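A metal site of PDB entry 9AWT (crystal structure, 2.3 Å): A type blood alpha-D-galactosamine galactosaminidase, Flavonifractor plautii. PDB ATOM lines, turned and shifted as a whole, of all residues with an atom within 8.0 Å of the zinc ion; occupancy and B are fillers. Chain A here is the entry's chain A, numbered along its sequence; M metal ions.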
ATOM      1  N   GLU A 379      -0.726  24.623 -12.209  1.00  0.00           N
ATOM      2  CA  GLU A 379      -1.568  23.786 -13.060  1.00  0.00           C
ATOM      3  C   GLU A 379      -1.524  24.255 -14.512  1.00  0.00           C
ATOM      4  O   GLU A 379      -1.879  23.509 -15.415  1.00  0.00           O
ATOM      5  CB  GLU A 379      -3.000  23.707 -12.474  1.00  0.00           C
ATOM      6  CG  GLU A 379      -3.831  24.999 -12.531  1.00  0.00           C
ATOM      7  CD  GLU A 379      -3.641  26.047 -11.415  1.00  0.00           C
ATOM      8  OE1 GLU A 379      -4.376  27.088 -11.451  1.00  0.00           O
ATOM      9  OE2 GLU A 379      -2.755  25.847 -10.539  1.00  0.00           O
ATOM     10  N   TYR A 380      -1.053  25.484 -14.789  1.00  0.00           N
ATOM     11  CA  TYR A 380      -0.896  25.971 -16.146  1.00  0.00           C
ATOM     12  C   TYR A 380       0.334  25.410 -16.863  1.00  0.00           C
ATOM     13  O   TYR A 380       0.478  25.565 -18.081  1.00  0.00           O
ATOM     14  CB  TYR A 380      -0.806  27.499 -16.222  1.00  0.00           C
ATOM     15  CG  TYR A 380      -1.972  28.321 -15.679  1.00  0.00           C
ATOM     16  CD1 TYR A 380      -3.176  27.733 -15.269  1.00  0.00           C
ATOM     17  CD2 TYR A 380      -1.862  29.704 -15.567  1.00  0.00           C
ATOM     18  CE1 TYR A 380      -4.214  28.503 -14.749  1.00  0.00           C
ATOM     19  CE2 TYR A 380      -2.890  30.490 -15.074  1.00  0.00           C
ATOM     20  CZ  TYR A 380      -4.073  29.878 -14.674  1.00  0.00           C
ATOM     21  OH  TYR A 380      -5.054  30.656 -14.162  1.00  0.00           O
ATOM     22  N   PHE A 381       1.244  24.765 -16.146  1.00  0.00           N
ATOM     23  CA  PHE A 381       2.570  24.470 -16.662  1.00  0.00           C
ATOM     24  C   PHE A 381       2.646  23.010 -17.104  1.00  0.00           C
ATOM     25  O   PHE A 381       1.807  22.197 -16.701  1.00  0.00           O
ATOM     26  CB  PHE A 381       3.623  24.783 -15.601  1.00  0.00           C
ATOM     27  CG  PHE A 381       3.852  26.264 -15.329  1.00  0.00           C
ATOM     28  CD1 PHE A 381       5.016  26.894 -15.743  1.00  0.00           C
ATOM     29  CD2 PHE A 381       2.898  27.024 -14.656  1.00  0.00           C
ATOM     30  CE1 PHE A 381       5.230  28.235 -15.483  1.00  0.00           C
ATOM     31  CE2 PHE A 381       3.103  28.380 -14.412  1.00  0.00           C
ATOM     32  CZ  PHE A 381       4.273  28.977 -14.836  1.00  0.00           C
ATOM     33  N   VAL A 382       3.678  22.686 -17.907  1.00  0.00           N
ATOM     34  CA  VAL A 382       3.961  21.319 -18.296  1.00  0.00           C
ATOM     35  C   VAL A 382       4.555  20.564 -17.096  1.00  0.00           C
ATOM     36  O   VAL A 382       5.388  21.117 -16.392  1.00  0.00           O
ATOM     37  CB  VAL A 382       4.924  21.278 -19.495  1.00  0.00           C
ATOM     38  CG1 VAL A 382       5.358  19.857 -19.829  1.00  0.00           C
ATOM     39  CG2 VAL A 382       4.377  21.957 -20.738  1.00  0.00           C
ATOM     40  N   MET A 383       4.148  19.295 -16.930  1.00  0.00           N
ATOM     41  CA  MET A 383       4.598  18.416 -15.863  1.00  0.00           C
ATOM     42  C   MET A 383       5.339  17.225 -16.491  1.00  0.00           C
ATOM     43  O   MET A 383       4.854  16.619 -17.459  1.00  0.00           O
ATOM     44  CB  MET A 383       3.404  17.935 -15.026  1.00  0.00           C
ATOM     45  CG  MET A 383       3.776  17.066 -13.822  1.00  0.00           C
ATOM     46  SD  MET A 383       2.374  16.498 -12.813  1.00  0.00           S
ATOM     47  CE  MET A 383       1.950  17.966 -11.852  1.00  0.00           C
ATOM     48  N   ALA A 406       8.091  25.610 -18.759  1.00  0.00           N
ATOM     49  CA  ALA A 406       7.234  25.643 -19.921  1.00  0.00           C
ATOM     50  C   ALA A 406       5.751  25.739 -19.561  1.00  0.00           C
ATOM     51  O   ALA A 406       5.263  24.980 -18.712  1.00  0.00           O
ATOM     52  CB  ALA A 406       7.495  24.397 -20.749  1.00  0.00           C
ATOM     53  N   LEU A 407       5.046  26.645 -20.233  1.00  0.00           N
ATOM     54  CA  LEU A 407       3.593  26.693 -20.167  1.00  0.00           C
ATOM     55  C   LEU A 407       3.012  25.611 -21.086  1.00  0.00           C
ATOM     56  O   LEU A 407       3.491  25.419 -22.213  1.00  0.00           O
ATOM     57  CB  LEU A 407       3.073  28.074 -20.577  1.00  0.00           C
ATOM     58  CG  LEU A 407       3.414  29.234 -19.630  1.00  0.00           C
ATOM     59  CD1 LEU A 407       3.211  30.568 -20.305  1.00  0.00           C
ATOM     60  CD2 LEU A 407       2.590  29.144 -18.350  1.00  0.00           C
ATOM     61  N   CYS A 408       1.985  24.906 -20.598  1.00  0.00           N
ATOM     62  CA  CYS A 408       1.322  23.903 -21.407  1.00  0.00           C
ATOM     63  C   CYS A 408       0.372  24.583 -22.390  1.00  0.00           C
ATOM     64  O   CYS A 408      -0.501  25.336 -21.971  1.00  0.00           O
ATOM     65  CB  CYS A 408       0.553  22.874 -20.584  1.00  0.00           C
ATOM     66  SG  CYS A 408      -0.184  21.582 -21.604  1.00  0.00           S
ATOM     67  N   PRO A 409       0.535  24.355 -23.712  1.00  0.00           N
ATOM     68  CA  PRO A 409      -0.298  25.010 -24.716  1.00  0.00           C
ATOM     69  C   PRO A 409      -1.781  24.658 -24.667  1.00  0.00           C
ATOM     70  O   PRO A 409      -2.587  25.392 -25.224  1.00  0.00           O
ATOM     71  CB  PRO A 409       0.372  24.637 -26.051  1.00  0.00           C
ATOM     72  CG  PRO A 409       1.178  23.405 -25.737  1.00  0.00           C
ATOM     73  CD  PRO A 409       1.580  23.507 -24.292  1.00  0.00           C
ATOM     74  N   MET A 410      -2.155  23.605 -23.946  1.00  0.00           N
ATOM     75  CA  MET A 410      -3.558  23.216 -23.803  1.00  0.00           C
ATOM     76  C   MET A 410      -4.188  23.709 -22.495  1.00  0.00           C
ATOM     77  O   MET A 410      -5.362  23.439 -22.223  1.00  0.00           O
ATOM     78  CB  MET A 410      -3.686  21.690 -23.898  1.00  0.00           C
ATOM     79  CG  MET A 410      -3.396  21.170 -25.306  1.00  0.00           C
ATOM     80  SD  MET A 410      -3.860  19.454 -25.611  1.00  0.00           S
ATOM     81  CE  MET A 410      -5.387  19.070 -24.746  1.00  0.00           C
ATOM     82  N   ALA A 411      -3.428  24.417 -21.640  1.00  0.00           N
ATOM     83  CA  ALA A 411      -4.036  24.958 -20.435  1.00  0.00           C
ATOM     84  C   ALA A 411      -4.584  26.344 -20.758  1.00  0.00           C
ATOM     85  O   ALA A 411      -3.841  27.195 -21.273  1.00  0.00           O
ATOM     86  CB  ALA A 411      -3.018  25.024 -19.314  1.00  0.00           C
ATOM     87  N   MET A 442       9.326  22.293 -27.032  1.00  0.00           N
ATOM     88  CA  MET A 442       8.339  22.251 -25.961  1.00  0.00           C
ATOM     89  C   MET A 442       8.326  20.834 -25.380  1.00  0.00           C
ATOM     90  O   MET A 442       8.168  19.876 -26.122  1.00  0.00           O
ATOM     91  CB  MET A 442       6.955  22.614 -26.509  1.00  0.00           C
ATOM     92  CG  MET A 442       5.747  22.264 -25.627  1.00  0.00           C
ATOM     93  SD  MET A 442       5.544  23.319 -24.184  1.00  0.00           S
ATOM     94  CE  MET A 442       5.268  24.955 -24.869  1.00  0.00           C
ATOM     95  N   PRO A 443       8.512  20.655 -24.066  1.00  0.00           N
ATOM     96  CA  PRO A 443       8.576  19.301 -23.497  1.00  0.00           C
ATOM     97  C   PRO A 443       7.214  18.605 -23.450  1.00  0.00           C
ATOM     98  O   PRO A 443       6.167  19.251 -23.525  1.00  0.00           O
ATOM     99  CB  PRO A 443       9.149  19.553 -22.089  1.00  0.00           C
ATOM    100  CG  PRO A 443       8.688  20.951 -21.740  1.00  0.00           C
ATOM    101  CD  PRO A 443       8.661  21.702 -23.053  1.00  0.00           C
ATOM    102  N   GLU A 444       7.277  17.270 -23.336  1.00  0.00           N
ATOM    103  CA  GLU A 444       6.123  16.408 -23.186  1.00  0.00           C
ATOM    104  C   GLU A 444       5.492  16.632 -21.822  1.00  0.00           C
ATOM    105  O   GLU A 444       6.196  16.857 -20.846  1.00  0.00           O
ATOM    106  CB  GLU A 444       6.582  14.953 -23.348  1.00  0.00           C
ATOM    107  CG  GLU A 444       7.054  14.622 -24.770  1.00  0.00           C
ATOM    108  CD  GLU A 444       7.546  13.200 -25.019  1.00  0.00           C
ATOM    109  OE1 GLU A 444       7.753  12.885 -26.224  1.00  0.00           O
ATOM    110  OE2 GLU A 444       7.815  12.444 -24.057  1.00  0.00           O
ATOM    111  N   CYS A 445       4.147  16.573 -21.774  1.00  0.00           N
ATOM    112  CA  CYS A 445       3.352  16.879 -20.589  1.00  0.00           C
ATOM    113  C   CYS A 445       2.654  15.629 -20.067  1.00  0.00           C
ATOM    114  O   CYS A 445       1.954  14.949 -20.829  1.00  0.00           O
ATOM    115  CB  CYS A 445       2.321  17.970 -20.869  1.00  0.00           C
ATOM    116  SG  CYS A 445       1.475  18.564 -19.368  1.00  0.00           S
ATOM    117  N   TYR A 446       2.817  15.347 -18.768  1.00  0.00           N
ATOM    118  CA  TYR A 446       2.264  14.164 -18.107  1.00  0.00           C
ATOM    119  C   TYR A 446       1.260  14.539 -17.005  1.00  0.00           C
ATOM    120  O   TYR A 446       0.898  13.698 -16.186  1.00  0.00           O
ATOM    121  CB  TYR A 446       3.379  13.331 -17.462  1.00  0.00           C
ATOM    122  CG  TYR A 446       4.305  12.659 -18.464  1.00  0.00           C
ATOM    123  CD1 TYR A 446       4.154  11.312 -18.804  1.00  0.00           C
ATOM    124  CD2 TYR A 446       5.306  13.377 -19.099  1.00  0.00           C
ATOM    125  CE1 TYR A 446       4.971  10.707 -19.738  1.00  0.00           C
ATOM    126  CE2 TYR A 446       6.138  12.782 -20.033  1.00  0.00           C
ATOM    127  CZ  TYR A 446       5.964  11.451 -20.358  1.00  0.00           C
ATOM    128  OH  TYR A 446       6.803  10.909 -21.301  1.00  0.00           O
ATOM    129  N   ASN A 447       0.791  15.789 -16.984  1.00  0.00           N
ATOM    130  CA  ASN A 447      -0.143  16.192 -15.948  1.00  0.00           C
ATOM    131  C   ASN A 447      -1.512  15.573 -16.221  1.00  0.00           C
ATOM    132  O   ASN A 447      -2.165  15.942 -17.177  1.00  0.00           O
ATOM    133  CB  ASN A 447      -0.261  17.709 -15.847  1.00  0.00           C
ATOM    134  CG  ASN A 447      -1.090  18.124 -14.657  1.00  0.00           C
ATOM    135  OD1 ASN A 447      -1.971  17.392 -14.203  1.00  0.00           O
ATOM    136  ND2 ASN A 447      -0.832  19.326 -14.174  1.00  0.00           N
ATOM    137  N   PRO A 448      -2.006  14.650 -15.362  1.00  0.00           N
ATOM    138  CA  PRO A 448      -3.245  13.921 -15.651  1.00  0.00           C
ATOM    139  C   PRO A 448      -4.476  14.816 -15.700  1.00  0.00           C
ATOM    140  O   PRO A 448      -5.442  14.508 -16.390  1.00  0.00           O
ATOM    141  CB  PRO A 448      -3.314  12.838 -14.563  1.00  0.00           C
ATOM    142  CG  PRO A 448      -2.488  13.394 -13.426  1.00  0.00           C
ATOM    143  CD  PRO A 448      -1.440  14.301 -14.043  1.00  0.00           C
ATOM    144  N   ALA A 449      -4.423  15.962 -15.001  1.00  0.00           N
ATOM    145  CA  ALA A 449      -5.524  16.913 -14.986  1.00  0.00           C
ATOM    146  C   ALA A 449      -5.683  17.633 -16.327  1.00  0.00           C
ATOM    147  O   ALA A 449      -6.725  18.266 -16.562  1.00  0.00           O
ATOM    148  CB  ALA A 449      -5.331  17.893 -13.843  1.00  0.00           C
ATOM    149  N   HIS A 450      -4.676  17.563 -17.215  1.00  0.00           N
ATOM    150  CA  HIS A 450      -4.810  18.146 -18.552  1.00  0.00           C
ATOM    151  C   HIS A 450      -5.525  17.180 -19.520  1.00  0.00           C
ATOM    152  O   HIS A 450      -5.957  17.627 -20.585  1.00  0.00           O
ATOM    153  CB  HIS A 450      -3.453  18.584 -19.119  1.00  0.00           C
ATOM    154  CG  HIS A 450      -2.758  19.674 -18.353  1.00  0.00           C
ATOM    155  ND1 HIS A 450      -1.497  20.109 -18.665  1.00  0.00           N
ATOM    156  CD2 HIS A 450      -3.153  20.414 -17.298  1.00  0.00           C
ATOM    157  CE1 HIS A 450      -1.142  21.071 -17.825  1.00  0.00           C
ATOM    158  NE2 HIS A 450      -2.134  21.268 -16.980  1.00  0.00           N
ATOM    159  N   ASN A 451      -5.595  15.879 -19.180  1.00  0.00           N
ATOM    160  CA  ASN A 451      -6.282  14.882 -20.005  1.00  0.00           C
ATOM    161  C   ASN A 451      -5.691  14.817 -21.417  1.00  0.00           C
ATOM    162  O   ASN A 451      -6.432  14.868 -22.395  1.00  0.00           O
ATOM    163  CB  ASN A 451      -7.781  15.138 -20.151  1.00  0.00           C
ATOM    164  CG  ASN A 451      -8.529  14.992 -18.840  1.00  0.00           C
ATOM    165  OD1 ASN A 451      -8.557  13.893 -18.284  1.00  0.00           O
ATOM    166  ND2 ASN A 451      -9.101  16.072 -18.324  1.00  0.00           N
ATOM    167  N   HIS A 452      -4.371  14.697 -21.537  1.00  0.00           N
ATOM    168  CA  HIS A 452      -3.721  14.672 -22.837  1.00  0.00           C
ATOM    169  C   HIS A 452      -3.985  13.331 -23.541  1.00  0.00           C
ATOM    170  O   HIS A 452      -3.993  12.288 -22.914  1.00  0.00           O
ATOM    171  CB  HIS A 452      -2.226  14.988 -22.718  1.00  0.00           C
ATOM    172  CG  HIS A 452      -1.852  16.392 -22.375  1.00  0.00           C
ATOM    173  ND1 HIS A 452      -2.044  17.429 -23.263  1.00  0.00           N
ATOM    174  CD2 HIS A 452      -1.262  16.943 -21.277  1.00  0.00           C
ATOM    175  CE1 HIS A 452      -1.610  18.581 -22.714  1.00  0.00           C
ATOM    176  NE2 HIS A 452      -1.099  18.295 -21.517  1.00  0.00           N
ATOM    177  N   SER A 454      -1.868  12.039 -25.623  1.00  0.00           N
ATOM    178  CA  SER A 454      -0.570  11.411 -25.435  1.00  0.00           C
ATOM    179  C   SER A 454       0.379  12.440 -24.828  1.00  0.00           C
ATOM    180  O   SER A 454       0.105  13.634 -24.901  1.00  0.00           O
ATOM    181  CB  SER A 454      -0.009  10.876 -26.733  1.00  0.00           C
ATOM    182  OG  SER A 454       0.366  11.980 -27.560  1.00  0.00           O
ATOM    183  N   PRO A 455       1.523  12.058 -24.234  1.00  0.00           N
ATOM    184  CA  PRO A 455       2.482  13.056 -23.741  1.00  0.00           C
ATOM    185  C   PRO A 455       3.079  14.005 -24.783  1.00  0.00           C
ATOM    186  O   PRO A 455       3.411  15.127 -24.431  1.00  0.00           O
ATOM    187  CB  PRO A 455       3.549  12.171 -23.041  1.00  0.00           C
ATOM    188  CG  PRO A 455       2.823  10.861 -22.724  1.00  0.00           C
ATOM    189  CD  PRO A 455       1.901  10.672 -23.924  1.00  0.00           C
ATOM    190  N   GLU A 457       1.492  15.536 -27.051  1.00  0.00           N
ATOM    191  CA  GLU A 457       0.493  16.486 -27.493  1.00  0.00           C
ATOM    192  C   GLU A 457       0.947  17.922 -27.185  1.00  0.00           C
ATOM    193  O   GLU A 457       0.706  18.824 -27.981  1.00  0.00           O
ATOM    194  CB  GLU A 457      -0.846  16.088 -26.844  1.00  0.00           C
ATOM    195  CG  GLU A 457      -2.039  16.920 -27.333  1.00  0.00           C
ATOM    196  CD  GLU A 457      -3.400  16.509 -26.781  1.00  0.00           C
ATOM    197  OE1 GLU A 457      -4.358  16.457 -27.561  1.00  0.00           O
ATOM    198  OE2 GLU A 457      -3.503  16.246 -25.583  1.00  0.00           O
ATOM    199  N   SER A 458       1.610  18.152 -26.052  1.00  0.00           N
ATOM    200  CA  SER A 458       2.123  19.475 -25.733  1.00  0.00           C
ATOM    201  C   SER A 458       3.101  19.946 -26.807  1.00  0.00           C
ATOM    202  O   SER A 458       2.963  21.051 -27.331  1.00  0.00           O
ATOM    203  CB  SER A 458       2.742  19.500 -24.355  1.00  0.00           C
ATOM    204  OG  SER A 458       3.671  18.427 -24.185  1.00  0.00           O
HETATM  205 ZN    ZN M   1      -0.236  19.644 -20.253  1.00  0.00          ZN
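The side-chain sulfur (SD) of Met 410 lies within hydrogen-bond range of a ring nitrogen (ND1) of His 452. A ring nitrogen (NE2) of His 450 is in hydrogen-bond range of the backbone carbonyl oxygen of Glu 379 (2.7 Å). The side-chain sulfur (SG) of Cys 445 sits close to the backbone NH (N) of Asn 447 (3.7 Å). N of Cys 445 lies within hydrogen-bond range of OG of Ser 458 (3.1 Å). The side-chain sulfur (SG) of Cys 445 lies close to the backbone NH (N) of Met 383 (3.7 Å). The backbone NH (N) of Cys 445 sits at hydrogen-bond distance from the backbone carbonyl oxygen (O) of Pro 455 (3.1 Å). SG of Cys 408 lies close to N of Met 410, 3.7 Å away. The backbone NH (N) of Cys 408 lies within hydrogen-bond range of the backbone carbonyl oxygen (O) of Tyr 380 (3.0 Å).
Of the 26 residues printed, 4 come within 4 Å of the zinc ion. The nearest printed residue that does not touch the zinc ion is Asn 447 (4.8 Å).
The zinc ion is bound by a ring nitrogen (NE2) of His 452 (2.0 Å), a ring nitrogen (ND1) of His 450 (2.1 Å), the side-chain sulfur (SG) of Cys 445 (2.2 Å) and the side-chain sulfur (SG) of Cys 408 (2.4 Å).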
